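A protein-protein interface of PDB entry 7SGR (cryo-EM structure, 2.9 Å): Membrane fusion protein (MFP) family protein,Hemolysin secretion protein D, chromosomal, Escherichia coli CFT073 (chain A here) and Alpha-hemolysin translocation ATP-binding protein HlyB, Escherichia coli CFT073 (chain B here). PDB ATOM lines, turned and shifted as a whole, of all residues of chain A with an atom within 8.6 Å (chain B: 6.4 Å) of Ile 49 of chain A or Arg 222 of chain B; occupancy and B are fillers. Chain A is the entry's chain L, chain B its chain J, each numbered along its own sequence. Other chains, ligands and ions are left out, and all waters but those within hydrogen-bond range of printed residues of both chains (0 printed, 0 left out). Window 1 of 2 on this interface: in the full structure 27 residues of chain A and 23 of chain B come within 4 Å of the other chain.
O of Val 53 of chain A sits at hydrogen-bond distance from NH2 of Arg 58 of chain A (2.7 Å).
NZ of Lys 149 of chain B lies within hydrogen-bond range of OH of Tyr 150 of chain B (3.2 Å).
Ile 49 of chain A touches four residues of chain B.
Of the printed residues of chain A, Arg 222 of chain B touches Leu 48 (3.2 Å), Ile 49 (2.9 Å), Glu 50 (3.97 Å), Thr 51 (3.5 Å) and Pro 52 (3.9 Å).
Of the printed residues of chain A, Val 225 of chain B touches His 45, Leu 48 and Ile 49.
Of the printed residues of chain B, Val 53 of chain A touches His 218 (3.4 Å).
Printed residues of chain A within 4 Å of Lys 149 of chain B: Thr 31 (3.8 Å) and Ile 49 (3.9 Å).
Of the printed residues of chain B, His 45 of chain A touches Val 225.
Of the printed residues of chain B, Glu 50 of chain A touches Arg 222.
Glu 226 of chain B touches none of the printed residues of chain A.
Leu 227 of chain B touches none of the printed residues of chain A.
The nearest residue of chain A that does not touch Arg 222 of chain B is Val 53 of chain A (4.7 Å).
Val 225 of chain B touches His 45 of chain A (CG1 to O, 3.9 Å).
CG2 of Val 225 of chain B touches CD2 of Leu 48 of chain A, at 3.9 Å.
Ile 49 of chain A touches Lys 149 of chain B.
Val 225 of chain B touches Ile 49 of chain A (CG1 to CG1, 3.7 Å).
Arg 222 of chain B touches Glu 50 of chain A.
His 218 of chain B touches Thr 51 of chain A.
Thr 51 of chain A touches Arg 222 of chain B (O to CZ, 3.5 Å).
His 218 of chain B touches Pro 52 of chain A (CE1 to O, 3.7 Å).
NH1 of Arg 222 of chain B touches CA of Pro 52 of chain A, 3.9 Å away.
Val 53 of chain A touches His 218 of chain B (CG2 to ND1, 3.4 Å).
OH of Tyr 150 of chain B lies within hydrogen-bond range of O of Ile 49 of chain A, at 3.4 Å.
The guanidinium group (NE) of Arg 222 of chain B is in hydrogen-bond range of the backbone carbonyl oxygen (O) of Ile 49 of chain A, 2.9 Å away.
Of the 17 printed residues of chain A, 8 touch a printed residue of chain B.
Hydrophobic or aromatic side chains of chain A within 4 Å of the printed part of chain B: Leu 48, Ile 49 and Val 53.
Of the 15 printed residues of chain B, 5 touch a printed residue of chain A.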
ATOM      1  N   THR A  31      29.048   2.028  -2.830  1.00  0.00           N
ATOM      2  CA  THR A  31      28.298   2.646  -3.911  1.00  0.00           C
ATOM      3  C   THR A  31      29.249   3.295  -4.913  1.00  0.00           C
ATOM      4  O   THR A  31      30.364   3.689  -4.554  1.00  0.00           O
ATOM      5  CB  THR A  31      27.339   3.699  -3.359  1.00  0.00           C
ATOM      6  OG1 THR A  31      28.078   4.698  -2.645  1.00  0.00           O
ATOM      7  CG2 THR A  31      26.328   3.057  -2.421  1.00  0.00           C
ATOM      8  N   PRO A  32      28.844   3.410  -6.178  1.00  0.00           N
ATOM      9  CA  PRO A  32      29.720   4.041  -7.173  1.00  0.00           C
ATOM     10  C   PRO A  32      29.974   5.506  -6.845  1.00  0.00           C
ATOM     11  O   PRO A  32      29.128   6.189  -6.265  1.00  0.00           O
ATOM     12  CB  PRO A  32      28.941   3.885  -8.485  1.00  0.00           C
ATOM     13  CG  PRO A  32      27.960   2.787  -8.228  1.00  0.00           C
ATOM     14  CD  PRO A  32      27.604   2.894  -6.781  1.00  0.00           C
ATOM     15  N   ASN A  39      24.748  13.495  -7.527  1.00  0.00           N
ATOM     16  CA  ASN A  39      24.249  13.120  -6.208  1.00  0.00           C
ATOM     17  C   ASN A  39      23.034  13.955  -5.825  1.00  0.00           C
ATOM     18  O   ASN A  39      22.099  13.458  -5.190  1.00  0.00           O
ATOM     19  CB  ASN A  39      25.353  13.272  -5.161  1.00  0.00           C
ATOM     20  CG  ASN A  39      26.309  12.099  -5.146  1.00  0.00           C
ATOM     21  OD1 ASN A  39      25.950  10.988  -5.534  1.00  0.00           O
ATOM     22  ND2 ASN A  39      27.532  12.339  -4.692  1.00  0.00           N
ATOM     23  N   LEU A  42      18.783  12.906  -7.207  1.00  0.00           N
ATOM     24  CA  LEU A  42      18.472  11.512  -6.931  1.00  0.00           C
ATOM     25  C   LEU A  42      17.142  11.468  -6.202  1.00  0.00           C
ATOM     26  O   LEU A  42      16.590  12.511  -5.837  1.00  0.00           O
ATOM     27  CB  LEU A  42      19.576  10.872  -6.074  1.00  0.00           C
ATOM     28  CG  LEU A  42      20.756  10.215  -6.789  1.00  0.00           C
ATOM     29  CD1 LEU A  42      21.837   9.864  -5.785  1.00  0.00           C
ATOM     30  CD2 LEU A  42      20.304   8.981  -7.542  1.00  0.00           C
ATOM     31  N   PRO A  43      16.577  10.270  -5.989  1.00  0.00           N
ATOM     32  CA  PRO A  43      15.435  10.166  -5.072  1.00  0.00           C
ATOM     33  C   PRO A  43      15.753  10.767  -3.712  1.00  0.00           C
ATOM     34  O   PRO A  43      16.921  10.836  -3.320  1.00  0.00           O
ATOM     35  CB  PRO A  43      15.194   8.656  -4.993  1.00  0.00           C
ATOM     36  CG  PRO A  43      15.600   8.169  -6.334  1.00  0.00           C
ATOM     37  CD  PRO A  43      16.767   9.028  -6.761  1.00  0.00           C
ATOM     38  N   ALA A  44      14.720  11.204  -2.988  1.00  0.00           N
ATOM     39  CA  ALA A  44      14.939  12.053  -1.820  1.00  0.00           C
ATOM     40  C   ALA A  44      15.783  11.357  -0.759  1.00  0.00           C
ATOM     41  O   ALA A  44      16.703  11.961  -0.198  1.00  0.00           O
ATOM     42  CB  ALA A  44      13.597  12.490  -1.235  1.00  0.00           C
ATOM     43  N   HIS A  45      15.494  10.087  -0.473  1.00  0.00           N
ATOM     44  CA  HIS A  45      16.247   9.380   0.558  1.00  0.00           C
ATOM     45  C   HIS A  45      17.624   8.957   0.060  1.00  0.00           C
ATOM     46  O   HIS A  45      18.594   8.956   0.829  1.00  0.00           O
ATOM     47  CB  HIS A  45      15.461   8.162   1.045  1.00  0.00           C
ATOM     48  CG  HIS A  45      15.204   7.139  -0.017  1.00  0.00           C
ATOM     49  ND1 HIS A  45      14.557   7.434  -1.197  1.00  0.00           N
ATOM     50  CD2 HIS A  45      15.505   5.820  -0.074  1.00  0.00           C
ATOM     51  CE1 HIS A  45      14.473   6.342  -1.936  1.00  0.00           C
ATOM     52  NE2 HIS A  45      15.041   5.349  -1.277  1.00  0.00           N
ATOM     53  N   LEU A  46      17.729   8.598  -1.221  1.00  0.00           N
ATOM     54  CA  LEU A  46      19.000   8.111  -1.743  1.00  0.00           C
ATOM     55  C   LEU A  46      20.054   9.207  -1.796  1.00  0.00           C
ATOM     56  O   LEU A  46      21.250   8.909  -1.732  1.00  0.00           O
ATOM     57  CB  LEU A  46      18.805   7.496  -3.126  1.00  0.00           C
ATOM     58  CG  LEU A  46      18.063   6.162  -3.156  1.00  0.00           C
ATOM     59  CD1 LEU A  46      17.712   5.776  -4.580  1.00  0.00           C
ATOM     60  CD2 LEU A  46      18.898   5.081  -2.496  1.00  0.00           C
ATOM     61  N   GLU A  47      19.646  10.474  -1.909  1.00  0.00           N
ATOM     62  CA  GLU A  47      20.649  11.530  -1.989  1.00  0.00           C
ATOM     63  C   GLU A  47      21.121  11.957  -0.605  1.00  0.00           C
ATOM     64  O   GLU A  47      22.103  12.696  -0.489  1.00  0.00           O
ATOM     65  CB  GLU A  47      20.115  12.715  -2.797  1.00  0.00           C
ATOM     66  CG  GLU A  47      18.890  13.429  -2.264  1.00  0.00           C
ATOM     67  CD  GLU A  47      19.228  14.509  -1.261  1.00  0.00           C
ATOM     68  OE1 GLU A  47      20.392  14.959  -1.245  1.00  0.00           O
ATOM     69  OE2 GLU A  47      18.318  14.948  -0.530  1.00  0.00           O
ATOM     70  N   LEU A  48      20.437  11.512   0.455  1.00  0.00           N
ATOM     71  CA  LEU A  48      21.043  11.558   1.782  1.00  0.00           C
ATOM     72  C   LEU A  48      21.898  10.326   2.038  1.00  0.00           C
ATOM     73  O   LEU A  48      22.966  10.426   2.650  1.00  0.00           O
ATOM     74  CB  LEU A  48      19.983  11.677   2.880  1.00  0.00           C
ATOM     75  CG  LEU A  48      19.298  13.010   3.184  1.00  0.00           C
ATOM     76  CD1 LEU A  48      18.337  13.408   2.096  1.00  0.00           C
ATOM     77  CD2 LEU A  48      18.585  12.939   4.522  1.00  0.00           C
ATOM     78  N   ILE A  49      21.441   9.160   1.580  1.00  0.00           N
ATOM     79  CA  ILE A  49      22.180   7.926   1.829  1.00  0.00           C
ATOM     80  C   ILE A  49      23.531   7.937   1.124  1.00  0.00           C
ATOM     81  O   ILE A  49      24.540   7.504   1.696  1.00  0.00           O
ATOM     82  CB  ILE A  49      21.338   6.708   1.407  1.00  0.00           C
ATOM     83  CG1 ILE A  49      20.109   6.572   2.303  1.00  0.00           C
ATOM     84  CG2 ILE A  49      22.165   5.436   1.461  1.00  0.00           C
ATOM     85  CD1 ILE A  49      19.219   5.410   1.935  1.00  0.00           C
ATOM     86  N   GLU A  50      23.588   8.440  -0.108  1.00  0.00           N
ATOM     87  CA  GLU A  50      24.762   8.283  -0.953  1.00  0.00           C
ATOM     88  C   GLU A  50      25.634   9.527  -1.055  1.00  0.00           C
ATOM     89  O   GLU A  50      26.671   9.475  -1.724  1.00  0.00           O
ATOM     90  CB  GLU A  50      24.332   7.853  -2.363  1.00  0.00           C
ATOM     91  CG  GLU A  50      23.727   6.461  -2.413  1.00  0.00           C
ATOM     92  CD  GLU A  50      23.291   6.064  -3.805  1.00  0.00           C
ATOM     93  OE1 GLU A  50      23.346   6.919  -4.713  1.00  0.00           O
ATOM     94  OE2 GLU A  50      22.888   4.897  -3.993  1.00  0.00           O
ATOM     95  N   THR A  51      25.255  10.633  -0.423  1.00  0.00           N
ATOM     96  CA  THR A  51      26.082  11.832  -0.483  1.00  0.00           C
ATOM     97  C   THR A  51      27.169  11.778   0.583  1.00  0.00           C
ATOM     98  O   THR A  51      26.862  11.720   1.780  1.00  0.00           O
ATOM     99  CB  THR A  51      25.236  13.093  -0.306  1.00  0.00           C
ATOM    100  OG1 THR A  51      24.186  13.105  -1.280  1.00  0.00           O
ATOM    101  CG2 THR A  51      26.092  14.334  -0.477  1.00  0.00           C
ATOM    102  N   PRO A  52      28.437  11.800   0.195  1.00  0.00           N
ATOM    103  CA  PRO A  52      29.528  11.739   1.171  1.00  0.00           C
ATOM    104  C   PRO A  52      29.727  13.087   1.855  1.00  0.00           C
ATOM    105  O   PRO A  52      29.105  14.090   1.511  1.00  0.00           O
ATOM    106  CB  PRO A  52      30.734  11.359   0.313  1.00  0.00           C
ATOM    107  CG  PRO A  52      30.426  11.937  -1.017  1.00  0.00           C
ATOM    108  CD  PRO A  52      28.936  11.826  -1.189  1.00  0.00           C
ATOM    109  N   VAL A  53      30.619  13.090   2.847  1.00  0.00           N
ATOM    110  CA  VAL A  53      30.913  14.304   3.597  1.00  0.00           C
ATOM    111  C   VAL A  53      31.625  15.299   2.690  1.00  0.00           C
ATOM    112  O   VAL A  53      32.441  14.920   1.839  1.00  0.00           O
ATOM    113  CB  VAL A  53      31.758  13.969   4.838  1.00  0.00           C
ATOM    114  CG1 VAL A  53      32.165  15.232   5.581  1.00  0.00           C
ATOM    115  CG2 VAL A  53      30.999  13.027   5.756  1.00  0.00           C
ATOM    116  N   SER A  54      31.310  16.581   2.862  1.00  0.00           N
ATOM    117  CA  SER A  54      31.924  17.620   2.051  1.00  0.00           C
ATOM    118  C   SER A  54      33.437  17.632   2.249  1.00  0.00           C
ATOM    119  O   SER A  54      33.961  17.272   3.306  1.00  0.00           O
ATOM    120  CB  SER A  54      31.338  18.987   2.396  1.00  0.00           C
ATOM    121  OG  SER A  54      31.995  20.016   1.678  1.00  0.00           O
ATOM    122  N   ARG A  58      36.986  18.128   5.656  1.00  0.00           N
ATOM    123  CA  ARG A  58      38.032  17.113   5.671  1.00  0.00           C
ATOM    124  C   ARG A  58      39.409  17.743   5.507  1.00  0.00           C
ATOM    125  O   ARG A  58      40.345  17.403   6.241  1.00  0.00           O
ATOM    126  CB  ARG A  58      37.770  16.076   4.580  1.00  0.00           C
ATOM    127  CG  ARG A  58      38.319  14.698   4.902  1.00  0.00           C
ATOM    128  CD  ARG A  58      37.986  13.691   3.815  1.00  0.00           C
ATOM    129  NE  ARG A  58      36.562  13.669   3.505  1.00  0.00           N
ATOM    130  CZ  ARG A  58      36.066  13.563   2.280  1.00  0.00           C
ATOM    131  NH1 ARG A  58      36.853  13.464   1.222  1.00  0.00           N
ATOM    132  NH2 ARG A  58      34.746  13.556   2.112  1.00  0.00           N
ATOM    133  N   LYS B 149      30.296  -0.285   5.379  1.00  0.00           N
ATOM    134  CA  LYS B 149      30.093   0.459   4.141  1.00  0.00           C
ATOM    135  C   LYS B 149      30.662   1.869   4.245  1.00  0.00           C
ATOM    136  O   LYS B 149      31.179   2.411   3.262  1.00  0.00           O
ATOM    137  CB  LYS B 149      28.605   0.498   3.795  1.00  0.00           C
ATOM    138  CG  LYS B 149      28.274   1.257   2.526  1.00  0.00           C
ATOM    139  CD  LYS B 149      26.774   1.408   2.352  1.00  0.00           C
ATOM    140  CE  LYS B 149      26.446   2.494   1.342  1.00  0.00           C
ATOM    141  NZ  LYS B 149      24.987   2.793   1.293  1.00  0.00           N
ATOM    142  N   TYR B 150      30.583   2.475   5.429  1.00  0.00           N
ATOM    143  CA  TYR B 150      31.142   3.801   5.687  1.00  0.00           C
ATOM    144  C   TYR B 150      32.416   3.724   6.519  1.00  0.00           C
ATOM    145  O   TYR B 150      32.662   4.581   7.370  1.00  0.00           O
ATOM    146  CB  TYR B 150      30.109   4.686   6.376  1.00  0.00           C
ATOM    147  CG  TYR B 150      28.774   4.737   5.672  1.00  0.00           C
ATOM    148  CD1 TYR B 150      28.696   4.957   4.306  1.00  0.00           C
ATOM    149  CD2 TYR B 150      27.591   4.565   6.376  1.00  0.00           C
ATOM    150  CE1 TYR B 150      27.478   5.002   3.660  1.00  0.00           C
ATOM    151  CE2 TYR B 150      26.370   4.609   5.739  1.00  0.00           C
ATOM    152  CZ  TYR B 150      26.319   4.828   4.380  1.00  0.00           C
ATOM    153  OH  TYR B 150      25.104   4.873   3.739  1.00  0.00           O
ATOM    154  N   ILE B 153      35.265   6.720   6.487  1.00  0.00           N
ATOM    155  CA  ILE B 153      35.037   7.985   7.174  1.00  0.00           C
ATOM    156  C   ILE B 153      35.047   7.739   8.677  1.00  0.00           C
ATOM    157  O   ILE B 153      35.436   8.612   9.460  1.00  0.00           O
ATOM    158  CB  ILE B 153      33.727   8.647   6.707  1.00  0.00           C
ATOM    159  CG1 ILE B 153      33.664  10.100   7.178  1.00  0.00           C
ATOM    160  CG2 ILE B 153      32.513   7.866   7.179  1.00  0.00           C
ATOM    161  CD1 ILE B 153      34.674  10.999   6.507  1.00  0.00           C
ATOM    162  N   ALA B 217      28.003  12.962  12.991  1.00  0.00           N
ATOM    163  CA  ALA B 217      26.563  13.114  12.803  1.00  0.00           C
ATOM    164  C   ALA B 217      26.176  12.918  11.342  1.00  0.00           C
ATOM    165  O   ALA B 217      25.164  12.269  11.040  1.00  0.00           O
ATOM    166  CB  ALA B 217      26.110  14.485  13.301  1.00  0.00           C
ATOM    167  N   HIS B 218      26.974  13.465  10.422  1.00  0.00           N
ATOM    168  CA  HIS B 218      26.694  13.306   9.000  1.00  0.00           C
ATOM    169  C   HIS B 218      26.741  11.841   8.593  1.00  0.00           C
ATOM    170  O   HIS B 218      25.913  11.383   7.798  1.00  0.00           O
ATOM    171  CB  HIS B 218      27.692  14.129   8.184  1.00  0.00           C
ATOM    172  CG  HIS B 218      27.396  14.166   6.718  1.00  0.00           C
ATOM    173  ND1 HIS B 218      27.612  13.091   5.885  1.00  0.00           N
ATOM    174  CD2 HIS B 218      26.906  15.156   5.935  1.00  0.00           C
ATOM    175  CE1 HIS B 218      27.265  13.414   4.652  1.00  0.00           C
ATOM    176  NE2 HIS B 218      26.833  14.663   4.655  1.00  0.00           N
ATOM    177  N   SER B 219      27.705  11.089   9.125  1.00  0.00           N
ATOM    178  CA  SER B 219      27.812   9.673   8.795  1.00  0.00           C
ATOM    179  C   SER B 219      26.662   8.855   9.368  1.00  0.00           C
ATOM    180  O   SER B 219      26.167   7.944   8.696  1.00  0.00           O
ATOM    181  CB  SER B 219      29.147   9.118   9.290  1.00  0.00           C
ATOM    182  OG  SER B 219      30.232   9.802   8.689  1.00  0.00           O
ATOM    183  N   THR B 220      26.225   9.150  10.593  1.00  0.00           N
ATOM    184  CA  THR B 220      25.135   8.389  11.200  1.00  0.00           C
ATOM    185  C   THR B 220      23.760   8.746  10.641  1.00  0.00           C
ATOM    186  O   THR B 220      22.834   7.919  10.720  1.00  0.00           O
ATOM    187  CB  THR B 220      25.133   8.588  12.717  1.00  0.00           C
ATOM    188  OG1 THR B 220      25.372   9.967  13.021  1.00  0.00           O
ATOM    189  CG2 THR B 220      26.217   7.741  13.361  1.00  0.00           C
ATOM    190  N   SER B 221      23.603   9.950  10.081  1.00  0.00           N
ATOM    191  CA  SER B 221      22.324  10.319   9.485  1.00  0.00           C
ATOM    192  C   SER B 221      21.962   9.393   8.331  1.00  0.00           C
ATOM    193  O   SER B 221      20.797   9.007   8.176  1.00  0.00           O
ATOM    194  CB  SER B 221      22.362  11.772   9.018  1.00  0.00           C
ATOM    195  OG  SER B 221      22.333  12.658  10.123  1.00  0.00           O
ATOM    196  N   ARG B 222      22.946   9.024   7.511  1.00  0.00           N
ATOM    197  CA  ARG B 222      22.687   8.111   6.403  1.00  0.00           C
ATOM    198  C   ARG B 222      22.231   6.747   6.906  1.00  0.00           C
ATOM    199  O   ARG B 222      21.322   6.136   6.329  1.00  0.00           O
ATOM    200  CB  ARG B 222      23.940   7.982   5.541  1.00  0.00           C
ATOM    201  CG  ARG B 222      24.554   9.323   5.176  1.00  0.00           C
ATOM    202  CD  ARG B 222      26.048   9.219   4.951  1.00  0.00           C
ATOM    203  NE  ARG B 222      26.366   8.664   3.642  1.00  0.00           N
ATOM    204  CZ  ARG B 222      27.593   8.565   3.152  1.00  0.00           C
ATOM    205  NH1 ARG B 222      28.646   8.981   3.835  1.00  0.00           N
ATOM    206  NH2 ARG B 222      27.768   8.035   1.945  1.00  0.00           N
ATOM    207  N   ILE B 223      22.848   6.259   7.984  1.00  0.00           N
ATOM    208  CA  ILE B 223      22.455   4.972   8.549  1.00  0.00           C
ATOM    209  C   ILE B 223      21.012   5.020   9.034  1.00  0.00           C
ATOM    210  O   ILE B 223      20.225   4.098   8.777  1.00  0.00           O
ATOM    211  CB  ILE B 223      23.419   4.568   9.680  1.00  0.00           C
ATOM    212  CG1 ILE B 223      24.849   4.465   9.150  1.00  0.00           C
ATOM    213  CG2 ILE B 223      22.988   3.253  10.301  1.00  0.00           C
ATOM    214  CD1 ILE B 223      25.872   4.160  10.219  1.00  0.00           C
ATOM    215  N   ASP B 224      20.635   6.093   9.736  1.00  0.00           N
ATOM    216  CA  ASP B 224      19.259   6.141  10.227  1.00  0.00           C
ATOM    217  C   ASP B 224      18.257   6.331   9.090  1.00  0.00           C
ATOM    218  O   ASP B 224      17.137   5.813   9.167  1.00  0.00           O
ATOM    219  CB  ASP B 224      19.094   7.215  11.312  1.00  0.00           C
ATOM    220  CG  ASP B 224      19.263   8.631  10.794  1.00  0.00           C
ATOM    221  OD1 ASP B 224      18.578   9.028   9.830  1.00  0.00           O
ATOM    222  OD2 ASP B 224      20.070   9.370  11.394  1.00  0.00           O
ATOM    223  N   VAL B 225      18.638   7.042   8.024  1.00  0.00           N
ATOM    224  CA  VAL B 225      17.757   7.153   6.861  1.00  0.00           C
ATOM    225  C   VAL B 225      17.533   5.785   6.227  1.00  0.00           C
ATOM    226  O   VAL B 225      16.401   5.426   5.866  1.00  0.00           O
ATOM    227  CB  VAL B 225      18.332   8.153   5.842  1.00  0.00           C
ATOM    228  CG1 VAL B 225      17.592   8.047   4.522  1.00  0.00           C
ATOM    229  CG2 VAL B 225      18.240   9.562   6.375  1.00  0.00           C
ATOM    230  N   GLU B 226      18.607   5.009   6.066  1.00  0.00           N
ATOM    231  CA  GLU B 226      18.477   3.666   5.509  1.00  0.00           C
ATOM    232  C   GLU B 226      17.572   2.804   6.379  1.00  0.00           C
ATOM    233  O   GLU B 226      16.702   2.080   5.872  1.00  0.00           O
ATOM    234  CB  GLU B 226      19.859   3.030   5.367  1.00  0.00           C
ATOM    235  CG  GLU B 226      19.844   1.612   4.835  1.00  0.00           C
ATOM    236  CD  GLU B 226      21.239   1.066   4.613  1.00  0.00           C
ATOM    237  OE1 GLU B 226      22.214   1.810   4.856  1.00  0.00           O
ATOM    238  OE2 GLU B 226      21.363  -0.106   4.200  1.00  0.00           O
ATOM    239  N   LEU B 227      17.757   2.882   7.700  1.00  0.00           N
ATOM    240  CA  LEU B 227      16.915   2.113   8.610  1.00  0.00           C
ATOM    241  C   LEU B 227      15.451   2.508   8.475  1.00  0.00           C
ATOM    242  O   LEU B 227      14.570   1.642   8.458  1.00  0.00           O
ATOM    243  CB  LEU B 227      17.386   2.301  10.050  1.00  0.00           C
ATOM    244  CG  LEU B 227      16.618   1.505  11.107  1.00  0.00           C
ATOM    245  CD1 LEU B 227      16.514   0.041  10.713  1.00  0.00           C
ATOM    246  CD2 LEU B 227      17.273   1.651  12.468  1.00  0.00           C
ATOM    247  N   ALA B 229      13.850   3.899   5.855  1.00  0.00           N
ATOM    248  CA  ALA B 229      13.306   3.445   4.580  1.00  0.00           C
ATOM    249  C   ALA B 229      13.014   1.950   4.616  1.00  0.00           C
ATOM    250  O   ALA B 229      11.935   1.503   4.201  1.00  0.00           O
ATOM    251  CB  ALA B 229      14.273   3.783   3.446  1.00  0.00           C
